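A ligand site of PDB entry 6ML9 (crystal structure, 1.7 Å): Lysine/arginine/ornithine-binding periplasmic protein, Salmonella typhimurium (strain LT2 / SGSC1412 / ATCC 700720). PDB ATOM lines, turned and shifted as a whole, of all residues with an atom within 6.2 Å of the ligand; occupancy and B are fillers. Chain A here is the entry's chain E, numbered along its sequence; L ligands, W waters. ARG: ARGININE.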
ATOM      1  N   THR A  10      12.868  11.110  18.899  1.00  0.00           N
ATOM      2  CA  THR A  10      13.373  12.298  18.299  1.00  0.00           C
ATOM      3  C   THR A  10      13.216  12.214  16.774  1.00  0.00           C
ATOM      4  O   THR A  10      13.224  11.122  16.218  1.00  0.00           O
ATOM      5  CB  THR A  10      14.855  12.528  18.673  1.00  0.00           C
ATOM      6  OG1 THR A  10      15.272  13.819  18.256  1.00  0.00           O
ATOM      7  CG2 THR A  10      15.772  11.474  18.021  1.00  0.00           C
ATOM      8  N   ASP A  11      13.074  13.357  16.126  1.00  0.00           N
ATOM      9  CA  ASP A  11      13.211  13.456  14.666  1.00  0.00           C
ATOM     10  C   ASP A  11      14.666  13.794  14.371  1.00  0.00           C
ATOM     11  O   ASP A  11      15.282  14.604  15.073  1.00  0.00           O
ATOM     12  CB  ASP A  11      12.264  14.513  14.064  1.00  0.00           C
ATOM     13  CG  ASP A  11      12.838  15.171  12.833  1.00  0.00           C
ATOM     14  OD1 ASP A  11      12.559  14.695  11.718  1.00  0.00           O
ATOM     15  OD2 ASP A  11      13.607  16.135  12.992  1.00  0.00           O
ATOM     16  N   THR A  12      15.223  13.198  13.333  1.00  0.00           N
ATOM     17  CA  THR A  12      16.651  13.368  13.025  1.00  0.00           C
ATOM     18  C   THR A  12      16.907  14.210  11.763  1.00  0.00           C
ATOM     19  O   THR A  12      17.863  13.955  11.006  1.00  0.00           O
ATOM     20  CB  THR A  12      17.319  11.994  12.916  1.00  0.00           C
ATOM     21  OG1 THR A  12      16.659  11.248  11.909  1.00  0.00           O
ATOM     22  CG2 THR A  12      17.220  11.222  14.249  1.00  0.00           C
ATOM     23  N   THR A  13      16.085  15.244  11.553  1.00  0.00           N
ATOM     24  CA  THR A  13      16.295  16.170  10.430  1.00  0.00           C
ATOM     25  C   THR A  13      16.393  17.617  10.894  1.00  0.00           C
ATOM     26  O   THR A  13      16.001  18.542  10.198  1.00  0.00           O
ATOM     27  CB  THR A  13      15.162  16.035   9.368  1.00  0.00           C
ATOM     28  OG1 THR A  13      13.878  16.359   9.920  1.00  0.00           O
ATOM     29  CG2 THR A  13      15.139  14.626   8.832  1.00  0.00           C
ATOM     30  N   TYR A  14      16.960  17.791  12.086  1.00  0.00           N
ATOM     31  CA  TYR A  14      17.027  19.115  12.715  1.00  0.00           C
ATOM     32  C   TYR A  14      18.402  19.393  13.334  1.00  0.00           C
ATOM     33  O   TYR A  14      18.527  19.671  14.534  1.00  0.00           O
ATOM     34  CB  TYR A  14      15.920  19.222  13.775  1.00  0.00           C
ATOM     35  CG  TYR A  14      15.038  20.468  13.696  1.00  0.00           C
ATOM     36  CD1 TYR A  14      14.306  20.776  12.544  1.00  0.00           C
ATOM     37  CD2 TYR A  14      14.911  21.314  14.787  1.00  0.00           C
ATOM     38  CE1 TYR A  14      13.462  21.855  12.491  1.00  0.00           C
ATOM     39  CE2 TYR A  14      14.088  22.415  14.734  1.00  0.00           C
ATOM     40  CZ  TYR A  14      13.373  22.695  13.596  1.00  0.00           C
ATOM     41  OH  TYR A  14      12.520  23.768  13.540  1.00  0.00           O
ATOM     42  N   SER A  18      19.353  17.509  16.538  1.00  0.00           N
ATOM     43  CA  SER A  18      19.245  16.069  16.349  1.00  0.00           C
ATOM     44  C   SER A  18      19.249  15.765  14.866  1.00  0.00           C
ATOM     45  O   SER A  18      18.384  16.216  14.091  1.00  0.00           O
ATOM     46  CB  SER A  18      17.990  15.540  17.032  1.00  0.00           C
ATOM     47  OG  SER A  18      16.866  16.263  16.644  1.00  0.00           O
ATOM     48  N   PHE A  52       8.478  14.025  13.174  1.00  0.00           N
ATOM     49  CA  PHE A  52       8.181  14.902  14.277  1.00  0.00           C
ATOM     50  C   PHE A  52       6.714  14.826  14.681  1.00  0.00           C
ATOM     51  O   PHE A  52       6.395  14.839  15.867  1.00  0.00           O
ATOM     52  CB  PHE A  52       8.576  16.333  13.924  1.00  0.00           C
ATOM     53  CG  PHE A  52       8.415  17.289  15.060  1.00  0.00           C
ATOM     54  CD1 PHE A  52       9.350  17.333  16.066  1.00  0.00           C
ATOM     55  CD2 PHE A  52       7.303  18.086  15.150  1.00  0.00           C
ATOM     56  CE1 PHE A  52       9.200  18.179  17.149  1.00  0.00           C
ATOM     57  CE2 PHE A  52       7.139  18.967  16.234  1.00  0.00           C
ATOM     58  CZ  PHE A  52       8.106  18.998  17.214  1.00  0.00           C
ATOM     59  N   LEU A  55       5.656  12.182  17.257  1.00  0.00           N
ATOM     60  CA  LEU A  55       6.271  12.088  18.586  1.00  0.00           C
ATOM     61  C   LEU A  55       5.231  12.166  19.701  1.00  0.00           C
ATOM     62  O   LEU A  55       5.211  11.303  20.591  1.00  0.00           O
ATOM     63  CB  LEU A  55       7.324  13.203  18.755  1.00  0.00           C
ATOM     64  CG  LEU A  55       8.564  12.983  17.891  1.00  0.00           C
ATOM     65  CD1 LEU A  55       9.442  14.217  17.827  1.00  0.00           C
ATOM     66  CD2 LEU A  55       9.354  11.783  18.432  1.00  0.00           C
ATOM     67  N   SER A  69      13.588  16.580  21.195  1.00  0.00           N
ATOM     68  CA  SER A  69      13.504  16.839  19.771  1.00  0.00           C
ATOM     69  C   SER A  69      13.167  18.297  19.457  1.00  0.00           C
ATOM     70  O   SER A  69      12.388  18.559  18.538  1.00  0.00           O
ATOM     71  CB  SER A  69      12.445  15.933  19.172  1.00  0.00           C
ATOM     72  OG  SER A  69      12.589  15.843  17.765  1.00  0.00           O
ATOM     73  N   SER A  70      13.780  19.207  20.216  1.00  0.00           N
ATOM     74  CA  SER A  70      13.496  20.641  20.133  1.00  0.00           C
ATOM     75  C   SER A  70      12.001  20.907  20.262  1.00  0.00           C
ATOM     76  O   SER A  70      11.435  21.759  19.556  1.00  0.00           O
ATOM     77  CB  SER A  70      14.028  21.235  18.828  1.00  0.00           C
ATOM     78  OG  SER A  70      15.427  21.123  18.796  1.00  0.00           O
ATOM     79  N   LEU A  71      11.361  20.196  21.199  1.00  0.00           N
ATOM     80  CA  LEU A  71       9.915  20.301  21.418  1.00  0.00           C
ATOM     81  C   LEU A  71       9.578  21.498  22.294  1.00  0.00           C
ATOM     82  O   LEU A  71       9.828  21.486  23.494  1.00  0.00           O
ATOM     83  CB  LEU A  71       9.378  19.018  22.091  1.00  0.00           C
ATOM     84  CG  LEU A  71       7.869  18.885  22.218  1.00  0.00           C
ATOM     85  CD1 LEU A  71       7.258  18.656  20.861  1.00  0.00           C
ATOM     86  CD2 LEU A  71       7.519  17.756  23.174  1.00  0.00           C
ATOM     87  N   SER A  72       9.044  22.542  21.678  1.00  0.00           N
ATOM     88  CA  SER A  72       8.721  23.781  22.385  1.00  0.00           C
ATOM     89  C   SER A  72       7.624  23.558  23.412  1.00  0.00           C
ATOM     90  O   SER A  72       6.625  22.890  23.138  1.00  0.00           O
ATOM     91  CB  SER A  72       8.291  24.857  21.407  1.00  0.00           C
ATOM     92  OG  SER A  72       9.394  25.246  20.603  1.00  0.00           O
ATOM     93  N   ILE A  73       7.827  24.193  24.562  1.00  0.00           N
ATOM     94  CA  ILE A  73       6.890  24.154  25.665  1.00  0.00           C
ATOM     95  C   ILE A  73       5.792  25.186  25.400  1.00  0.00           C
ATOM     96  O   ILE A  73       6.019  26.377  25.595  1.00  0.00           O
ATOM     97  CB  ILE A  73       7.589  24.474  26.985  1.00  0.00           C
ATOM     98  CG1 ILE A  73       8.799  23.567  27.183  1.00  0.00           C
ATOM     99  CG2 ILE A  73       6.674  24.328  28.182  1.00  0.00           C
ATOM    100  CD1 ILE A  73       9.716  24.023  28.291  1.00  0.00           C
ATOM    101  N   ARG A  77       0.317  22.464  24.092  1.00  0.00           N
ATOM    102  CA  ARG A  77       0.871  21.134  24.361  1.00  0.00           C
ATOM    103  C   ARG A  77       0.744  20.723  25.825  1.00  0.00           C
ATOM    104  O   ARG A  77       0.601  19.542  26.113  1.00  0.00           O
ATOM    105  CB  ARG A  77       2.325  21.065  23.933  1.00  0.00           C
ATOM    106  CG  ARG A  77       2.480  21.007  22.424  1.00  0.00           C
ATOM    107  CD  ARG A  77       3.938  21.099  22.009  1.00  0.00           C
ATOM    108  NE  ARG A  77       4.053  20.939  20.570  1.00  0.00           N
ATOM    109  CZ  ARG A  77       5.070  21.372  19.848  1.00  0.00           C
ATOM    110  NH1 ARG A  77       6.067  21.995  20.446  1.00  0.00           N
ATOM    111  NH2 ARG A  77       5.104  21.181  18.524  1.00  0.00           N
ATOM    112  N   ALA A  90      14.164  28.632  21.747  1.00  0.00           N
ATOM    113  CA  ALA A  90      13.922  28.384  20.331  1.00  0.00           C
ATOM    114  C   ALA A  90      12.968  29.395  19.735  1.00  0.00           C
ATOM    115  O   ALA A  90      11.759  29.246  19.851  1.00  0.00           O
ATOM    116  CB  ALA A  90      13.374  26.972  20.122  1.00  0.00           C
ATOM    117  N   SER A  92      11.583  31.264  16.138  1.00  0.00           N
ATOM    118  CA  SER A  92      11.295  30.891  14.753  1.00  0.00           C
ATOM    119  C   SER A  92      11.680  32.044  13.831  1.00  0.00           C
ATOM    120  O   SER A  92      11.522  33.232  14.171  1.00  0.00           O
ATOM    121  CB  SER A  92       9.819  30.554  14.550  1.00  0.00           C
ATOM    122  OG  SER A  92       9.485  29.361  15.228  1.00  0.00           O
ATOM    123  N   LEU A 117       7.216  22.381   8.936  1.00  0.00           N
ATOM    124  CA  LEU A 117       7.196  21.000   9.410  1.00  0.00           C
ATOM    125  C   LEU A 117       5.851  20.557   9.982  1.00  0.00           C
ATOM    126  O   LEU A 117       5.315  21.225  10.882  1.00  0.00           O
ATOM    127  CB  LEU A 117       8.286  20.829  10.464  1.00  0.00           C
ATOM    128  CG  LEU A 117       8.434  19.479  11.127  1.00  0.00           C
ATOM    129  CD1 LEU A 117       8.896  18.400  10.128  1.00  0.00           C
ATOM    130  CD2 LEU A 117       9.434  19.663  12.244  1.00  0.00           C
ATOM    131  N   GLY A 119       3.164  19.118  12.228  1.00  0.00           N
ATOM    132  CA  GLY A 119       3.141  18.878  13.658  1.00  0.00           C
ATOM    133  C   GLY A 119       3.881  19.937  14.475  1.00  0.00           C
ATOM    134  O   GLY A 119       3.900  19.871  15.712  1.00  0.00           O
ATOM    135  N   SER A 120       4.513  20.884  13.800  1.00  0.00           N
ATOM    136  CA  SER A 120       5.299  21.916  14.506  1.00  0.00           C
ATOM    137  C   SER A 120       4.494  23.142  14.878  1.00  0.00           C
ATOM    138  O   SER A 120       3.406  23.406  14.365  1.00  0.00           O
ATOM    139  CB  SER A 120       6.487  22.373  13.649  1.00  0.00           C
ATOM    140  OG  SER A 120       6.056  23.128  12.536  1.00  0.00           O
ATOM    141  N   THR A 121       5.057  23.912  15.818  1.00  0.00           N
ATOM    142  CA  THR A 121       4.520  25.214  16.151  1.00  0.00           C
ATOM    143  C   THR A 121       4.542  26.141  14.936  1.00  0.00           C
ATOM    144  O   THR A 121       3.671  26.981  14.796  1.00  0.00           O
ATOM    145  CB  THR A 121       5.324  25.880  17.250  1.00  0.00           C
ATOM    146  OG1 THR A 121       6.698  25.922  16.850  1.00  0.00           O
ATOM    147  CG2 THR A 121       5.204  25.136  18.545  1.00  0.00           C
ATOM    148  N   GLN A 122       5.527  25.958  14.052  1.00  0.00           N
ATOM    149  CA  GLN A 122       5.578  26.768  12.850  1.00  0.00           C
ATOM    150  C   GLN A 122       4.398  26.464  11.950  1.00  0.00           C
ATOM    151  O   GLN A 122       3.831  27.353  11.318  1.00  0.00           O
ATOM    152  CB  GLN A 122       6.875  26.567  12.112  1.00  0.00           C
ATOM    153  CG  GLN A 122       8.069  27.134  12.860  1.00  0.00           C
ATOM    154  CD  GLN A 122       8.725  26.152  13.806  1.00  0.00           C
ATOM    155  OE1 GLN A 122       8.389  24.962  13.850  1.00  0.00           O
ATOM    156  NE2 GLN A 122       9.662  26.654  14.612  1.00  0.00           N
ATOM    157  N   GLN A 143      12.100  18.050   8.014  1.00  0.00           N
ATOM    158  CA  GLN A 143      12.732  19.310   7.640  1.00  0.00           C
ATOM    159  C   GLN A 143      13.709  19.173   6.459  1.00  0.00           C
ATOM    160  O   GLN A 143      13.971  20.165   5.752  1.00  0.00           O
ATOM    161  CB  GLN A 143      13.466  19.916   8.844  1.00  0.00           C
ATOM    162  CG  GLN A 143      14.026  21.324   8.620  1.00  0.00           C
ATOM    163  CD  GLN A 143      13.004  22.433   8.531  1.00  0.00           C
ATOM    164  OE1 GLN A 143      11.929  22.398   9.169  1.00  0.00           O
ATOM    165  NE2 GLN A 143      13.326  23.440   7.764  1.00  0.00           N
ATOM    166  N   ASP A 161      12.800  26.625  13.378  1.00  0.00           N
ATOM    167  CA  ASP A 161      13.543  27.222  14.465  1.00  0.00           C
ATOM    168  C   ASP A 161      14.780  27.908  13.869  1.00  0.00           C
ATOM    169  O   ASP A 161      15.473  27.366  12.993  1.00  0.00           O
ATOM    170  CB  ASP A 161      13.967  26.183  15.531  1.00  0.00           C
ATOM    171  CG  ASP A 161      12.818  25.668  16.365  1.00  0.00           C
ATOM    172  OD1 ASP A 161      11.724  26.271  16.368  1.00  0.00           O
ATOM    173  OD2 ASP A 161      13.046  24.658  17.079  1.00  0.00           O
ATOM    174  N   PHE A 191       4.695  29.937  19.895  1.00  0.00           N
ATOM    175  CA  PHE A 191       6.016  29.330  19.877  1.00  0.00           C
ATOM    176  C   PHE A 191       6.510  28.891  21.246  1.00  0.00           C
ATOM    177  O   PHE A 191       7.530  28.193  21.361  1.00  0.00           O
ATOM    178  CB  PHE A 191       7.030  30.278  19.215  1.00  0.00           C
ATOM    179  CG  PHE A 191       6.682  30.581  17.790  1.00  0.00           C
ATOM    180  CD1 PHE A 191       6.518  29.546  16.860  1.00  0.00           C
ATOM    181  CD2 PHE A 191       6.446  31.863  17.375  1.00  0.00           C
ATOM    182  CE1 PHE A 191       6.169  29.811  15.556  1.00  0.00           C
ATOM    183  CE2 PHE A 191       6.098  32.122  16.079  1.00  0.00           C
ATOM    184  CZ  PHE A 191       5.959  31.099  15.166  1.00  0.00           C
ATOM    185  N   THR A 195      12.335  24.949  24.700  1.00  0.00           N
ATOM    186  CA  THR A 195      12.078  23.533  24.478  1.00  0.00           C
ATOM    187  C   THR A 195      12.240  22.768  25.787  1.00  0.00           C
ATOM    188  O   THR A 195      12.906  23.259  26.727  1.00  0.00           O
ATOM    189  CB  THR A 195      13.039  22.943  23.453  1.00  0.00           C
ATOM    190  OG1 THR A 195      14.348  23.013  24.001  1.00  0.00           O
ATOM    191  CG2 THR A 195      13.007  23.706  22.110  1.00  0.00           C
HETATM  192  N   ARG L   1      10.385  23.885  18.126  1.00  0.00           N
HETATM  193  CA  ARG L   1       9.420  23.545  17.056  1.00  0.00           C
HETATM  194  C   ARG L   1       8.275  22.783  17.695  1.00  0.00           C
HETATM  195  O   ARG L   1       8.358  22.468  18.910  1.00  0.00           O
HETATM  196  CB  ARG L   1      10.097  22.715  15.948  1.00  0.00           C
HETATM  197  CG  ARG L   1      10.812  21.487  16.470  1.00  0.00           C
HETATM  198  CD  ARG L   1      11.152  20.494  15.378  1.00  0.00           C
HETATM  199  NE  ARG L   1      12.083  19.486  15.846  1.00  0.00           N
HETATM  200  CZ  ARG L   1      12.589  18.516  15.086  1.00  0.00           C
HETATM  201  NH1 ARG L   1      12.244  18.394  13.809  1.00  0.00           N
HETATM  202  NH2 ARG L   1      13.424  17.632  15.605  1.00  0.00           N
HETATM  203  OXT ARG L   1       7.263  22.477  17.060  1.00  0.00           O
HETATM  204  O   HOH W   1      10.101  23.281  12.505  1.00  0.00           O
HETATM  205  O   HOH W   2      15.498  18.392  17.569  1.00  0.00           O
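Tyr 14 touches the ligand (CD1 to NH1, 3.4 Å). Ser 18 touches the ligand (OG to NH2, 3.8 Å). Phe 52 touches the ligand. CA of Leu 71 touches O of the ligand, at 3.7 Å. Leu 117 touches the ligand (CD2 to NH1, 3.5 Å). CA of Ser 120 touches OXT of the ligand, 3.3 Å away. Gln 122 touches the ligand. The nearest printed residue that does not touch the ligand is Gly 119 (4.5 Å).
N of the ligand sits at hydrogen-bond distance from O of Ser 70, 2.8 Å away. A nitrogen (NE) of the ligand sits at hydrogen-bond distance from the backbone carbonyl oxygen (O) of Ser 69 (2.9 Å). A nitrogen (NH1) of the ligand lies within salt-bridge range of the side-chain carboxylate (OD2) of Asp 11 (2.8 Å). The side-chain hydroxyl (OG1) of Thr 121 lies within hydrogen-bond range of an oxygen (OXT) of the ligand (3.5 Å). The side-chain carboxylate of Asp 161 is in salt-bridge range of a nitrogen (N) of the ligand, 3.0 Å away. The side-chain hydroxyl of Ser 72 lies within hydrogen-bond range of a nitrogen (N) of the ligand (3.0 Å). An oxygen (O) of the ligand lies within salt-bridge range of the guanidinium group (NH1) of Arg 77 (2.8 Å). N of Ser 72 lies within hydrogen-bond range of O of the ligand (2.9 Å). The backbone NH of Thr 121 sits at hydrogen-bond distance from an oxygen (OXT) of the ligand, at 2.9 Å. NH2 of the ligand sits at hydrogen-bond distance from OG of Ser 69 (2.9 Å).
Water W2 lies within hydrogen-bond range of OG of Ser 18 (2.7 Å), NH2 of the ligand (3.0 Å), OG of Ser 70 (3.0 Å) and O of Ser 69 (3.3 Å). Water W1 lies within hydrogen-bond range of OH of Tyr 14 (2.7 Å) and OE1 of Gln 122 (2.8 Å).
OD1 of Asp 161 is in hydrogen-bond range of NE2 of Gln 122 (2.7 Å). The side-chain hydroxyl (OG) of Ser 18 sits at hydrogen-bond distance from the side-chain hydroxyl (OG1) of Thr 10 (3.3 Å). The side-chain hydroxyl of Tyr 14 is in hydrogen-bond range of the backbone NH of Asp 161 (2.9 Å). O of Asp 11 lies within hydrogen-bond range of OG of Ser 18. The guanidinium group (NH2) of Arg 77 is in hydrogen-bond range of the backbone carbonyl oxygen (O) of Gly 119, 3.3 Å away. The side-chain amide nitrogen (NE2) of Gln 122 lies within hydrogen-bond range of the side-chain hydroxyl (OG) of Ser 92 (2.8 Å). The side-chain hydroxyl (OG) of Ser 120 sits close to the side-chain amide oxygen (OE1) of Gln 122 (3.2 Å). N of Asp 11 lies within hydrogen-bond range of OG of Ser 69, at 3.0 Å.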
